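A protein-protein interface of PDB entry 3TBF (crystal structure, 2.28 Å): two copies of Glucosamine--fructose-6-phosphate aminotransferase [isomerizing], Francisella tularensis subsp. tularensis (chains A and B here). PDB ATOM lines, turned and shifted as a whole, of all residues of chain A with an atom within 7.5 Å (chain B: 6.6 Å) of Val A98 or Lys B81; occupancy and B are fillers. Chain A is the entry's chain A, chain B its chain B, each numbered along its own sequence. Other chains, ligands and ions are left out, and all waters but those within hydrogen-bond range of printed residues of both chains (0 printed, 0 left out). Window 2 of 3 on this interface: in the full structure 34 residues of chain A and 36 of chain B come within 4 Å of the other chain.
The side-chain carboxylate of Glu B77 lies within salt-bridge range of the guanidinium group of Arg A95, 2.7 Å away. OE1 of Glu B77 is in hydrogen-bond range of N of Val A98.
N of Lys B81 is in hydrogen-bond range of O of Ile B76. NZ of Lys A123 lies within hydrogen-bond range of O of Arg A95 (2.7 Å). The side-chain amide oxygen (OE1) of Gln A127 sits close to the side-chain amide oxygen (OD1) of Asn A97 (3.2 Å). The backbone carbonyl oxygen (O) of Ile B76 lies within hydrogen-bond range of the backbone NH (N) of Val B82, at 3.4 Å. NZ of Lys B81 is in hydrogen-bond range of O of Lys B78. The backbone NH (N) of Cys B84 sits at hydrogen-bond distance from the side-chain carboxylate (OE2) of Glu B77 (2.9 Å).
C of Glu B77 touches O of Asp A96 (3.8 Å). Asp A96 touches Lys B78 (O to CA, 3.6 Å). Asn A97 touches Glu B77. Lys B81 touches Val A98. Val A98 touches Val B82 (CG2 to N, 3.9 Å). Pro B83 touches Val A98.
Of the printed residues of chain A, Lys B81 touches Val A98 (3.6 Å). No residue of chain A comes within 4 Å of Ala B80. Printed residues of chain A within 4 Å of Lys B78: Asp A96. Printed residues of chain B within 4 Å of Arg A95: Glu B77. The nearest printed residue of chain A that does not touch Lys B81 is Asp A96 (4.001 Å).
Of the 16 printed residues of chain A, 4 touch a printed residue of chain B. Among the printed residues, Asp or Glu carboxylates within 4 Å of a Lys or Arg side-chain nitrogen of the other chain: Arg A95 with Glu B77 (2.7 Å).
No position is printed for both chains. Of the 8 pairs that touch across the chains among the printed residues, none has its exchanged pair printed and touching as well.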
ATOM      1  N   HIS A  56      35.565  -1.710 -25.686  1.00  0.00           N
ATOM      2  CA  HIS A  56      36.096  -1.204 -24.482  1.00  0.00           C
ATOM      3  C   HIS A  56      37.268  -2.066 -24.124  1.00  0.00           C
ATOM      4  O   HIS A  56      37.257  -3.247 -24.303  1.00  0.00           O
ATOM      5  CB  HIS A  56      35.029  -1.284 -23.392  1.00  0.00           C
ATOM      6  CG  HIS A  56      35.477  -0.733 -22.082  1.00  0.00           C
ATOM      7  ND1 HIS A  56      36.162  -1.491 -21.159  1.00  0.00           N
ATOM      8  CD2 HIS A  56      35.322   0.496 -21.525  1.00  0.00           C
ATOM      9  CE1 HIS A  56      36.435  -0.746 -20.103  1.00  0.00           C
ATOM     10  NE2 HIS A  56      35.938   0.464 -20.298  1.00  0.00           N
ATOM     11  N   CYS A  58      39.843  -3.218 -21.081  1.00  0.00           N
ATOM     12  CA  CYS A  58      39.946  -3.357 -19.631  1.00  0.00           C
ATOM     13  C   CYS A  58      41.327  -3.863 -19.289  1.00  0.00           C
ATOM     14  O   CYS A  58      41.632  -5.043 -19.493  1.00  0.00           O
ATOM     15  CB  CYS A  58      38.894  -4.379 -19.126  1.00  0.00           C
ATOM     16  SG  CYS A  58      38.058  -3.967 -17.573  1.00  0.00           S
ATOM     17  N   SER A  85      39.767   1.304 -19.334  1.00  0.00           N
ATOM     18  CA  SER A  85      39.899   1.430 -17.904  1.00  0.00           C
ATOM     19  C   SER A  85      41.097   0.627 -17.394  1.00  0.00           C
ATOM     20  O   SER A  85      41.523  -0.375 -18.018  1.00  0.00           O
ATOM     21  CB  SER A  85      38.616   1.006 -17.190  1.00  0.00           C
ATOM     22  OG  SER A  85      38.376  -0.354 -17.399  1.00  0.00           O
ATOM     23  N   ILE A  92      40.374  -5.811  -8.473  1.00  0.00           N
ATOM     24  CA  ILE A  92      39.313  -6.242  -9.367  1.00  0.00           C
ATOM     25  C   ILE A  92      38.999  -7.700  -9.145  1.00  0.00           C
ATOM     26  O   ILE A  92      37.862  -8.151  -9.348  1.00  0.00           O
ATOM     27  CB  ILE A  92      39.597  -5.976 -10.860  1.00  0.00           C
ATOM     28  CG1 ILE A  92      38.323  -6.123 -11.697  1.00  0.00           C
ATOM     29  CG2 ILE A  92      40.695  -6.856 -11.432  1.00  0.00           C
ATOM     30  CD1 ILE A  92      38.662  -5.882 -13.208  1.00  0.00           C
ATOM     31  N   ARG A  95      36.370  -7.878  -6.433  1.00  0.00           N
ATOM     32  CA  ARG A  95      35.339  -6.871  -6.458  1.00  0.00           C
ATOM     33  C   ARG A  95      34.203  -7.323  -7.341  1.00  0.00           C
ATOM     34  O   ARG A  95      34.390  -8.025  -8.317  1.00  0.00           O
ATOM     35  CB  ARG A  95      35.915  -5.569  -6.989  1.00  0.00           C
ATOM     36  CG  ARG A  95      34.971  -4.437  -7.125  1.00  0.00           C
ATOM     37  CD  ARG A  95      35.716  -3.164  -7.409  1.00  0.00           C
ATOM     38  NE  ARG A  95      36.063  -2.944  -8.811  1.00  0.00           N
ATOM     39  CZ  ARG A  95      35.165  -2.707  -9.775  1.00  0.00           C
ATOM     40  NH1 ARG A  95      33.856  -2.691  -9.512  1.00  0.00           N
ATOM     41  NH2 ARG A  95      35.563  -2.519 -11.020  1.00  0.00           N
ATOM     42  N   ASP A  96      33.012  -6.871  -6.994  1.00  0.00           N
ATOM     43  CA  ASP A  96      31.822  -7.251  -7.700  1.00  0.00           C
ATOM     44  C   ASP A  96      31.598  -6.249  -8.852  1.00  0.00           C
ATOM     45  O   ASP A  96      30.823  -5.279  -8.700  1.00  0.00           O
ATOM     46  CB  ASP A  96      30.687  -7.239  -6.681  1.00  0.00           C
ATOM     47  CG  ASP A  96      29.547  -8.130  -7.071  1.00  0.00           C
ATOM     48  OD1 ASP A  96      29.324  -8.201  -8.305  1.00  0.00           O
ATOM     49  OD2 ASP A  96      28.878  -8.739  -6.158  1.00  0.00           O
ATOM     50  N   ASN A  97      32.283  -6.456  -9.981  1.00  0.00           N
ATOM     51  CA  ASN A  97      32.290  -5.484 -11.070  1.00  0.00           C
ATOM     52  C   ASN A  97      31.361  -5.823 -12.231  1.00  0.00           C
ATOM     53  O   ASN A  97      30.876  -6.950 -12.361  1.00  0.00           O
ATOM     54  CB  ASN A  97      33.693  -5.317 -11.626  1.00  0.00           C
ATOM     55  CG  ASN A  97      34.190  -6.567 -12.320  1.00  0.00           C
ATOM     56  OD1 ASN A  97      34.074  -7.676 -11.793  1.00  0.00           O
ATOM     57  ND2 ASN A  97      34.742  -6.398 -13.510  1.00  0.00           N
ATOM     58  N   VAL A  98      31.122  -4.798 -13.047  1.00  0.00           N
ATOM     59  CA  VAL A  98      30.276  -4.855 -14.206  1.00  0.00           C
ATOM     60  C   VAL A  98      31.156  -4.723 -15.438  1.00  0.00           C
ATOM     61  O   VAL A  98      32.065  -3.895 -15.507  1.00  0.00           O
ATOM     62  CB  VAL A  98      29.276  -3.687 -14.237  1.00  0.00           C
ATOM     63  CG1 VAL A  98      28.459  -3.708 -15.551  1.00  0.00           C
ATOM     64  CG2 VAL A  98      28.347  -3.705 -13.069  1.00  0.00           C
ATOM     65  N   VAL A  99      30.852  -5.511 -16.441  1.00  0.00           N
ATOM     66  CA  VAL A  99      31.659  -5.591 -17.624  1.00  0.00           C
ATOM     67  C   VAL A  99      30.888  -5.029 -18.795  1.00  0.00           C
ATOM     68  O   VAL A  99      29.902  -5.607 -19.214  1.00  0.00           O
ATOM     69  CB  VAL A  99      31.992  -7.039 -17.909  1.00  0.00           C
ATOM     70  CG1 VAL A  99      32.775  -7.153 -19.253  1.00  0.00           C
ATOM     71  CG2 VAL A  99      32.766  -7.607 -16.753  1.00  0.00           C
ATOM     72  N   VAL A 100      31.325  -3.892 -19.307  1.00  0.00           N
ATOM     73  CA  VAL A 100      30.731  -3.298 -20.519  1.00  0.00           C
ATOM     74  C   VAL A 100      30.627  -4.333 -21.686  1.00  0.00           C
ATOM     75  O   VAL A 100      31.520  -5.174 -21.879  1.00  0.00           O
ATOM     76  CB  VAL A 100      31.625  -2.100 -20.982  1.00  0.00           C
ATOM     77  CG1 VAL A 100      31.152  -1.557 -22.290  1.00  0.00           C
ATOM     78  CG2 VAL A 100      31.685  -0.969 -19.861  1.00  0.00           C
ATOM     79  N   ASP A 101      29.551  -4.293 -22.467  1.00  0.00           N
ATOM     80  CA  ASP A 101      29.519  -5.130 -23.686  1.00  0.00           C
ATOM     81  C   ASP A 101      30.725  -4.804 -24.585  1.00  0.00           C
ATOM     82  O   ASP A 101      31.124  -3.653 -24.728  1.00  0.00           O
ATOM     83  CB  ASP A 101      28.229  -4.936 -24.513  1.00  0.00           C
ATOM     84  CG  ASP A 101      27.092  -5.949 -24.159  1.00  0.00           C
ATOM     85  OD1 ASP A 101      27.330  -7.048 -23.578  1.00  0.00           O
ATOM     86  OD2 ASP A 101      25.922  -5.634 -24.500  1.00  0.00           O
ATOM     87  N   SER A 103      33.871  -5.723 -24.213  1.00  0.00           N
ATOM     88  CA  SER A 103      35.047  -5.442 -23.429  1.00  0.00           C
ATOM     89  C   SER A 103      36.146  -6.447 -23.703  1.00  0.00           C
ATOM     90  O   SER A 103      35.898  -7.648 -23.656  1.00  0.00           O
ATOM     91  CB  SER A 103      34.707  -5.502 -21.954  1.00  0.00           C
ATOM     92  OG  SER A 103      34.651  -4.209 -21.447  1.00  0.00           O
ATOM     93  N   LYS A 123      38.744 -15.339 -13.731  1.00  0.00           N
ATOM     94  CA  LYS A 123      37.433 -14.836 -13.405  1.00  0.00           C
ATOM     95  C   LYS A 123      36.757 -14.238 -14.636  1.00  0.00           C
ATOM     96  O   LYS A 123      35.570 -14.463 -14.874  1.00  0.00           O
ATOM     97  CB  LYS A 123      37.548 -13.839 -12.243  1.00  0.00           C
ATOM     98  CG  LYS A 123      36.476 -12.780 -12.177  1.00  0.00           C
ATOM     99  CD  LYS A 123      36.534 -11.943 -10.881  1.00  0.00           C
ATOM    100  CE  LYS A 123      36.036 -10.486 -11.168  1.00  0.00           C
ATOM    101  NZ  LYS A 123      35.510  -9.863  -9.945  1.00  0.00           N
ATOM    102  N   GLN A 127      32.715 -13.972 -17.400  1.00  0.00           N
ATOM    103  CA  GLN A 127      32.036 -12.684 -17.481  1.00  0.00           C
ATOM    104  C   GLN A 127      31.823 -12.324 -18.934  1.00  0.00           C
ATOM    105  O   GLN A 127      32.231 -13.029 -19.849  1.00  0.00           O
ATOM    106  CB  GLN A 127      32.822 -11.609 -16.711  1.00  0.00           C
ATOM    107  CG  GLN A 127      32.813 -11.843 -15.186  1.00  0.00           C
ATOM    108  CD  GLN A 127      33.578 -10.787 -14.369  1.00  0.00           C
ATOM    109  OE1 GLN A 127      33.026 -10.185 -13.429  1.00  0.00           O
ATOM    110  NE2 GLN A 127      34.845 -10.586 -14.698  1.00  0.00           N
ATOM    111  N   ASN A 128      31.192 -11.193 -19.141  1.00  0.00           N
ATOM    112  CA  ASN A 128      30.819 -10.744 -20.458  1.00  0.00           C
ATOM    113  C   ASN A 128      31.951 -10.198 -21.353  1.00  0.00           C
ATOM    114  O   ASN A 128      31.707  -9.306 -22.149  1.00  0.00           O
ATOM    115  CB  ASN A 128      29.780  -9.638 -20.256  1.00  0.00           C
ATOM    116  CG  ASN A 128      28.944  -9.389 -21.480  1.00  0.00           C
ATOM    117  OD1 ASN A 128      28.797 -10.282 -22.347  1.00  0.00           O
ATOM    118  ND2 ASN A 128      28.373  -8.175 -21.568  1.00  0.00           N
ATOM    119  N   TYR A 129      33.173 -10.681 -21.254  1.00  0.00           N
ATOM    120  CA  TYR A 129      34.212 -10.096 -22.127  1.00  0.00           C
ATOM    121  C   TYR A 129      34.180 -10.785 -23.483  1.00  0.00           C
ATOM    122  O   TYR A 129      33.806 -11.957 -23.565  1.00  0.00           O
ATOM    123  CB  TYR A 129      35.612 -10.267 -21.541  1.00  0.00           C
ATOM    124  CG  TYR A 129      35.860  -9.491 -20.281  1.00  0.00           C
ATOM    125  CD1 TYR A 129      36.238  -8.170 -20.335  1.00  0.00           C
ATOM    126  CD2 TYR A 129      35.737 -10.081 -19.040  1.00  0.00           C
ATOM    127  CE1 TYR A 129      36.498  -7.437 -19.191  1.00  0.00           C
ATOM    128  CE2 TYR A 129      35.976  -9.365 -17.888  1.00  0.00           C
ATOM    129  CZ  TYR A 129      36.370  -8.035 -17.972  1.00  0.00           C
ATOM    130  OH  TYR A 129      36.613  -7.313 -16.828  1.00  0.00           O
ATOM    131  N   LYS B  55      23.939   4.625 -19.067  1.00  0.00           N
ATOM    132  CA  LYS B  55      24.528   3.262 -19.190  1.00  0.00           C
ATOM    133  C   LYS B  55      25.899   3.140 -18.547  1.00  0.00           C
ATOM    134  O   LYS B  55      26.441   2.062 -18.410  1.00  0.00           O
ATOM    135  CB  LYS B  55      24.664   2.863 -20.643  1.00  0.00           C
ATOM    136  CG  LYS B  55      23.470   3.243 -21.509  1.00  0.00           C
ATOM    137  CD  LYS B  55      22.684   2.037 -22.045  1.00  0.00           C
ATOM    138  CE  LYS B  55      21.586   1.556 -21.051  1.00  0.00           C
ATOM    139  NZ  LYS B  55      20.426   2.532 -20.879  1.00  0.00           N
ATOM    140  N   TRP B  75      30.082   0.668  -4.739  1.00  0.00           N
ATOM    141  CA  TRP B  75      28.639   0.608  -4.527  1.00  0.00           C
ATOM    142  C   TRP B  75      27.862   0.568  -5.848  1.00  0.00           C
ATOM    143  O   TRP B  75      27.029  -0.275  -6.094  1.00  0.00           O
ATOM    144  CB  TRP B  75      28.189   1.849  -3.748  1.00  0.00           C
ATOM    145  CG  TRP B  75      28.616   1.923  -2.313  1.00  0.00           C
ATOM    146  CD1 TRP B  75      28.936   0.914  -1.537  1.00  0.00           C
ATOM    147  CD2 TRP B  75      28.710   3.097  -1.509  1.00  0.00           C
ATOM    148  NE1 TRP B  75      29.260   1.342  -0.287  1.00  0.00           N
ATOM    149  CE2 TRP B  75      29.090   2.693  -0.230  1.00  0.00           C
ATOM    150  CE3 TRP B  75      28.524   4.456  -1.754  1.00  0.00           C
ATOM    151  CZ2 TRP B  75      29.313   3.588   0.814  1.00  0.00           C
ATOM    152  CZ3 TRP B  75      28.711   5.342  -0.723  1.00  0.00           C
ATOM    153  CH2 TRP B  75      29.115   4.899   0.555  1.00  0.00           C
ATOM    154  N   ILE B  76      28.177   1.496  -6.721  1.00  0.00           N
ATOM    155  CA  ILE B  76      27.418   1.621  -7.942  1.00  0.00           C
ATOM    156  C   ILE B  76      27.500   0.356  -8.808  1.00  0.00           C
ATOM    157  O   ILE B  76      26.496  -0.092  -9.365  1.00  0.00           O
ATOM    158  CB  ILE B  76      27.902   2.781  -8.697  1.00  0.00           C
ATOM    159  CG1 ILE B  76      27.590   4.052  -7.912  1.00  0.00           C
ATOM    160  CG2 ILE B  76      27.280   2.829 -10.102  1.00  0.00           C
ATOM    161  CD1 ILE B  76      28.436   5.206  -8.454  1.00  0.00           C
ATOM    162  N   GLU B  77      28.697  -0.202  -8.933  1.00  0.00           N
ATOM    163  CA  GLU B  77      28.844  -1.384  -9.740  1.00  0.00           C
ATOM    164  C   GLU B  77      28.230  -2.599  -9.100  1.00  0.00           C
ATOM    165  O   GLU B  77      27.617  -3.363  -9.777  1.00  0.00           O
ATOM    166  CB  GLU B  77      30.312  -1.659 -10.062  1.00  0.00           C
ATOM    167  CG  GLU B  77      30.921  -0.607 -10.960  1.00  0.00           C
ATOM    168  CD  GLU B  77      31.958  -1.109 -11.963  1.00  0.00           C
ATOM    169  OE1 GLU B  77      32.500  -2.258 -11.862  1.00  0.00           O
ATOM    170  OE2 GLU B  77      32.222  -0.307 -12.897  1.00  0.00           O
ATOM    171  N   LYS B  78      28.347  -2.744  -7.793  1.00  0.00           N
ATOM    172  CA  LYS B  78      27.899  -3.907  -7.100  1.00  0.00           C
ATOM    173  C   LYS B  78      26.395  -3.918  -6.926  1.00  0.00           C
ATOM    174  O   LYS B  78      25.738  -4.957  -7.136  1.00  0.00           O
ATOM    175  CB  LYS B  78      28.541  -3.945  -5.707  1.00  0.00           C
ATOM    176  CG  LYS B  78      27.943  -4.967  -4.792  1.00  0.00           C
ATOM    177  CD  LYS B  78      28.804  -5.227  -3.556  1.00  0.00           C
ATOM    178  CE  LYS B  78      28.134  -6.345  -2.676  1.00  0.00           C
ATOM    179  NZ  LYS B  78      28.962  -6.770  -1.508  1.00  0.00           N
ATOM    180  N   TYR B  79      25.852  -2.785  -6.486  1.00  0.00           N
ATOM    181  CA  TYR B  79      24.443  -2.689  -6.159  1.00  0.00           C
ATOM    182  C   TYR B  79      23.588  -2.190  -7.329  1.00  0.00           C
ATOM    183  O   TYR B  79      22.531  -2.784  -7.624  1.00  0.00           O
ATOM    184  CB  TYR B  79      24.256  -1.815  -4.910  1.00  0.00           C
ATOM    185  CG  TYR B  79      24.778  -2.472  -3.643  1.00  0.00           C
ATOM    186  CD1 TYR B  79      24.063  -3.465  -3.013  1.00  0.00           C
ATOM    187  CD2 TYR B  79      26.002  -2.123  -3.102  1.00  0.00           C
ATOM    188  CE1 TYR B  79      24.524  -4.054  -1.852  1.00  0.00           C
ATOM    189  CE2 TYR B  79      26.486  -2.728  -1.969  1.00  0.00           C
ATOM    190  CZ  TYR B  79      25.733  -3.679  -1.329  1.00  0.00           C
ATOM    191  OH  TYR B  79      26.195  -4.292  -0.183  1.00  0.00           O
ATOM    192  N   ALA B  80      23.978  -1.104  -7.977  1.00  0.00           N
ATOM    193  CA  ALA B  80      23.201  -0.607  -9.124  1.00  0.00           C
ATOM    194  C   ALA B  80      23.519  -1.397 -10.397  1.00  0.00           C
ATOM    195  O   ALA B  80      22.778  -1.391 -11.379  1.00  0.00           O
ATOM    196  CB  ALA B  80      23.456   0.870  -9.339  1.00  0.00           C
ATOM    197  N   LYS B  81      24.637  -2.085 -10.369  1.00  0.00           N
ATOM    198  CA  LYS B  81      25.173  -2.776 -11.560  1.00  0.00           C
ATOM    199  C   LYS B  81      25.280  -1.890 -12.794  1.00  0.00           C
ATOM    200  O   LYS B  81      24.894  -2.277 -13.896  1.00  0.00           O
ATOM    201  CB  LYS B  81      24.389  -4.062 -11.836  1.00  0.00           C
ATOM    202  CG  LYS B  81      24.116  -4.778 -10.565  1.00  0.00           C
ATOM    203  CD  LYS B  81      23.999  -6.241 -10.712  1.00  0.00           C
ATOM    204  CE  LYS B  81      24.085  -6.950  -9.338  1.00  0.00           C
ATOM    205  NZ  LYS B  81      25.509  -7.099  -8.795  1.00  0.00           N
ATOM    206  N   VAL B  82      25.842  -0.709 -12.601  1.00  0.00           N
ATOM    207  CA  VAL B  82      26.120   0.182 -13.713  1.00  0.00           C
ATOM    208  C   VAL B  82      27.611   0.446 -13.698  1.00  0.00           C
ATOM    209  O   VAL B  82      28.197   0.724 -12.660  1.00  0.00           O
ATOM    210  CB  VAL B  82      25.362   1.508 -13.576  1.00  0.00           C
ATOM    211  CG1 VAL B  82      25.756   2.471 -14.662  1.00  0.00           C
ATOM    212  CG2 VAL B  82      23.833   1.264 -13.548  1.00  0.00           C
ATOM    213  N   PRO B  83      28.248   0.341 -14.855  1.00  0.00           N
ATOM    214  CA  PRO B  83      29.674   0.559 -14.898  1.00  0.00           C
ATOM    215  C   PRO B  83      29.979   2.015 -14.614  1.00  0.00           C
ATOM    216  O   PRO B  83      29.260   2.943 -15.036  1.00  0.00           O
ATOM    217  CB  PRO B  83      30.049   0.166 -16.320  1.00  0.00           C
ATOM    218  CG  PRO B  83      28.809   0.391 -17.077  1.00  0.00           C
ATOM    219  CD  PRO B  83      27.698   0.015 -16.176  1.00  0.00           C
ATOM    220  N   CYS B  84      31.079   2.202 -13.913  1.00  0.00           N
ATOM    221  CA  CYS B  84      31.388   3.475 -13.311  1.00  0.00           C
ATOM    222  C   CYS B  84      32.883   3.663 -13.416  1.00  0.00           C
ATOM    223  O   CYS B  84      33.632   2.724 -13.152  1.00  0.00           O
ATOM    224  CB  CYS B  84      30.943   3.438 -11.835  1.00  0.00           C
ATOM    225  SG  CYS B  84      31.287   4.909 -10.903  1.00  0.00           S
ATOM    226  N   THR B 178      22.989   5.694  -5.478  1.00  0.00           N
ATOM    227  CA  THR B 178      23.172   4.326  -5.924  1.00  0.00           C
ATOM    228  C   THR B 178      21.842   3.631  -5.866  1.00  0.00           C
ATOM    229  O   THR B 178      21.510   2.942  -6.819  1.00  0.00           O
ATOM    230  CB  THR B 178      24.180   3.613  -5.026  1.00  0.00           C
ATOM    231  OG1 THR B 178      25.438   4.287  -5.106  1.00  0.00           O
ATOM    232  CG2 THR B 178      24.380   2.197  -5.381  1.00  0.00           C
ATOM    233  N   ALA B 182      19.516   2.127  -8.714  1.00  0.00           N
ATOM    234  CA  ALA B 182      19.250   0.709  -8.596  1.00  0.00           C
ATOM    235  C   ALA B 182      17.776   0.313  -8.695  1.00  0.00           C
ATOM    236  O   ALA B 182      17.421  -0.657  -9.388  1.00  0.00           O
ATOM    237  CB  ALA B 182      19.811   0.223  -7.352  1.00  0.00           C
ATOM    238  N   LYS B 185      16.559   1.107 -12.321  1.00  0.00           N
ATOM    239  CA  LYS B 185      17.062   0.069 -13.242  1.00  0.00           C
ATOM    240  C   LYS B 185      16.667  -1.332 -12.829  1.00  0.00           C
ATOM    241  O   LYS B 185      16.978  -2.293 -13.513  1.00  0.00           O
ATOM    242  CB  LYS B 185      18.592   0.146 -13.370  1.00  0.00           C
ATOM    243  CG  LYS B 185      19.037   1.500 -13.854  1.00  0.00           C
ATOM    244  CD  LYS B 185      20.061   1.436 -14.908  1.00  0.00           C
ATOM    245  CE  LYS B 185      20.249   2.783 -15.623  1.00  0.00           C
ATOM    246  NZ  LYS B 185      19.402   2.966 -16.890  1.00  0.00           N
ATOM    247  N   SER B 187      17.873  -3.187 -10.497  1.00  0.00           N
ATOM    248  CA  SER B 187      19.040  -3.937 -10.077  1.00  0.00           C
ATOM    249  C   SER B 187      18.856  -4.593  -8.714  1.00  0.00           C
ATOM    250  O   SER B 187      19.483  -5.587  -8.403  1.00  0.00           O
ATOM    251  CB  SER B 187      20.209  -2.976 -10.006  1.00  0.00           C
ATOM    252  OG  SER B 187      20.461  -2.453 -11.304  1.00  0.00           O
ATOM    253  N   LEU B 188      18.006  -4.032  -7.885  1.00  0.00           N
ATOM    254  CA  LEU B 188      17.723  -4.651  -6.597  1.00  0.00           C
ATOM    255  C   LEU B 188      16.248  -4.791  -6.401  1.00  0.00           C
ATOM    256  O   LEU B 188      15.504  -4.024  -6.992  1.00  0.00           O
ATOM    257  CB  LEU B 188      18.272  -3.781  -5.503  1.00  0.00           C
ATOM    258  CG  LEU B 188      19.741  -3.467  -5.490  1.00  0.00           C
ATOM    259  CD1 LEU B 188      19.952  -2.298  -4.521  1.00  0.00           C
ATOM    260  CD2 LEU B 188      20.531  -4.733  -5.095  1.00  0.00           C
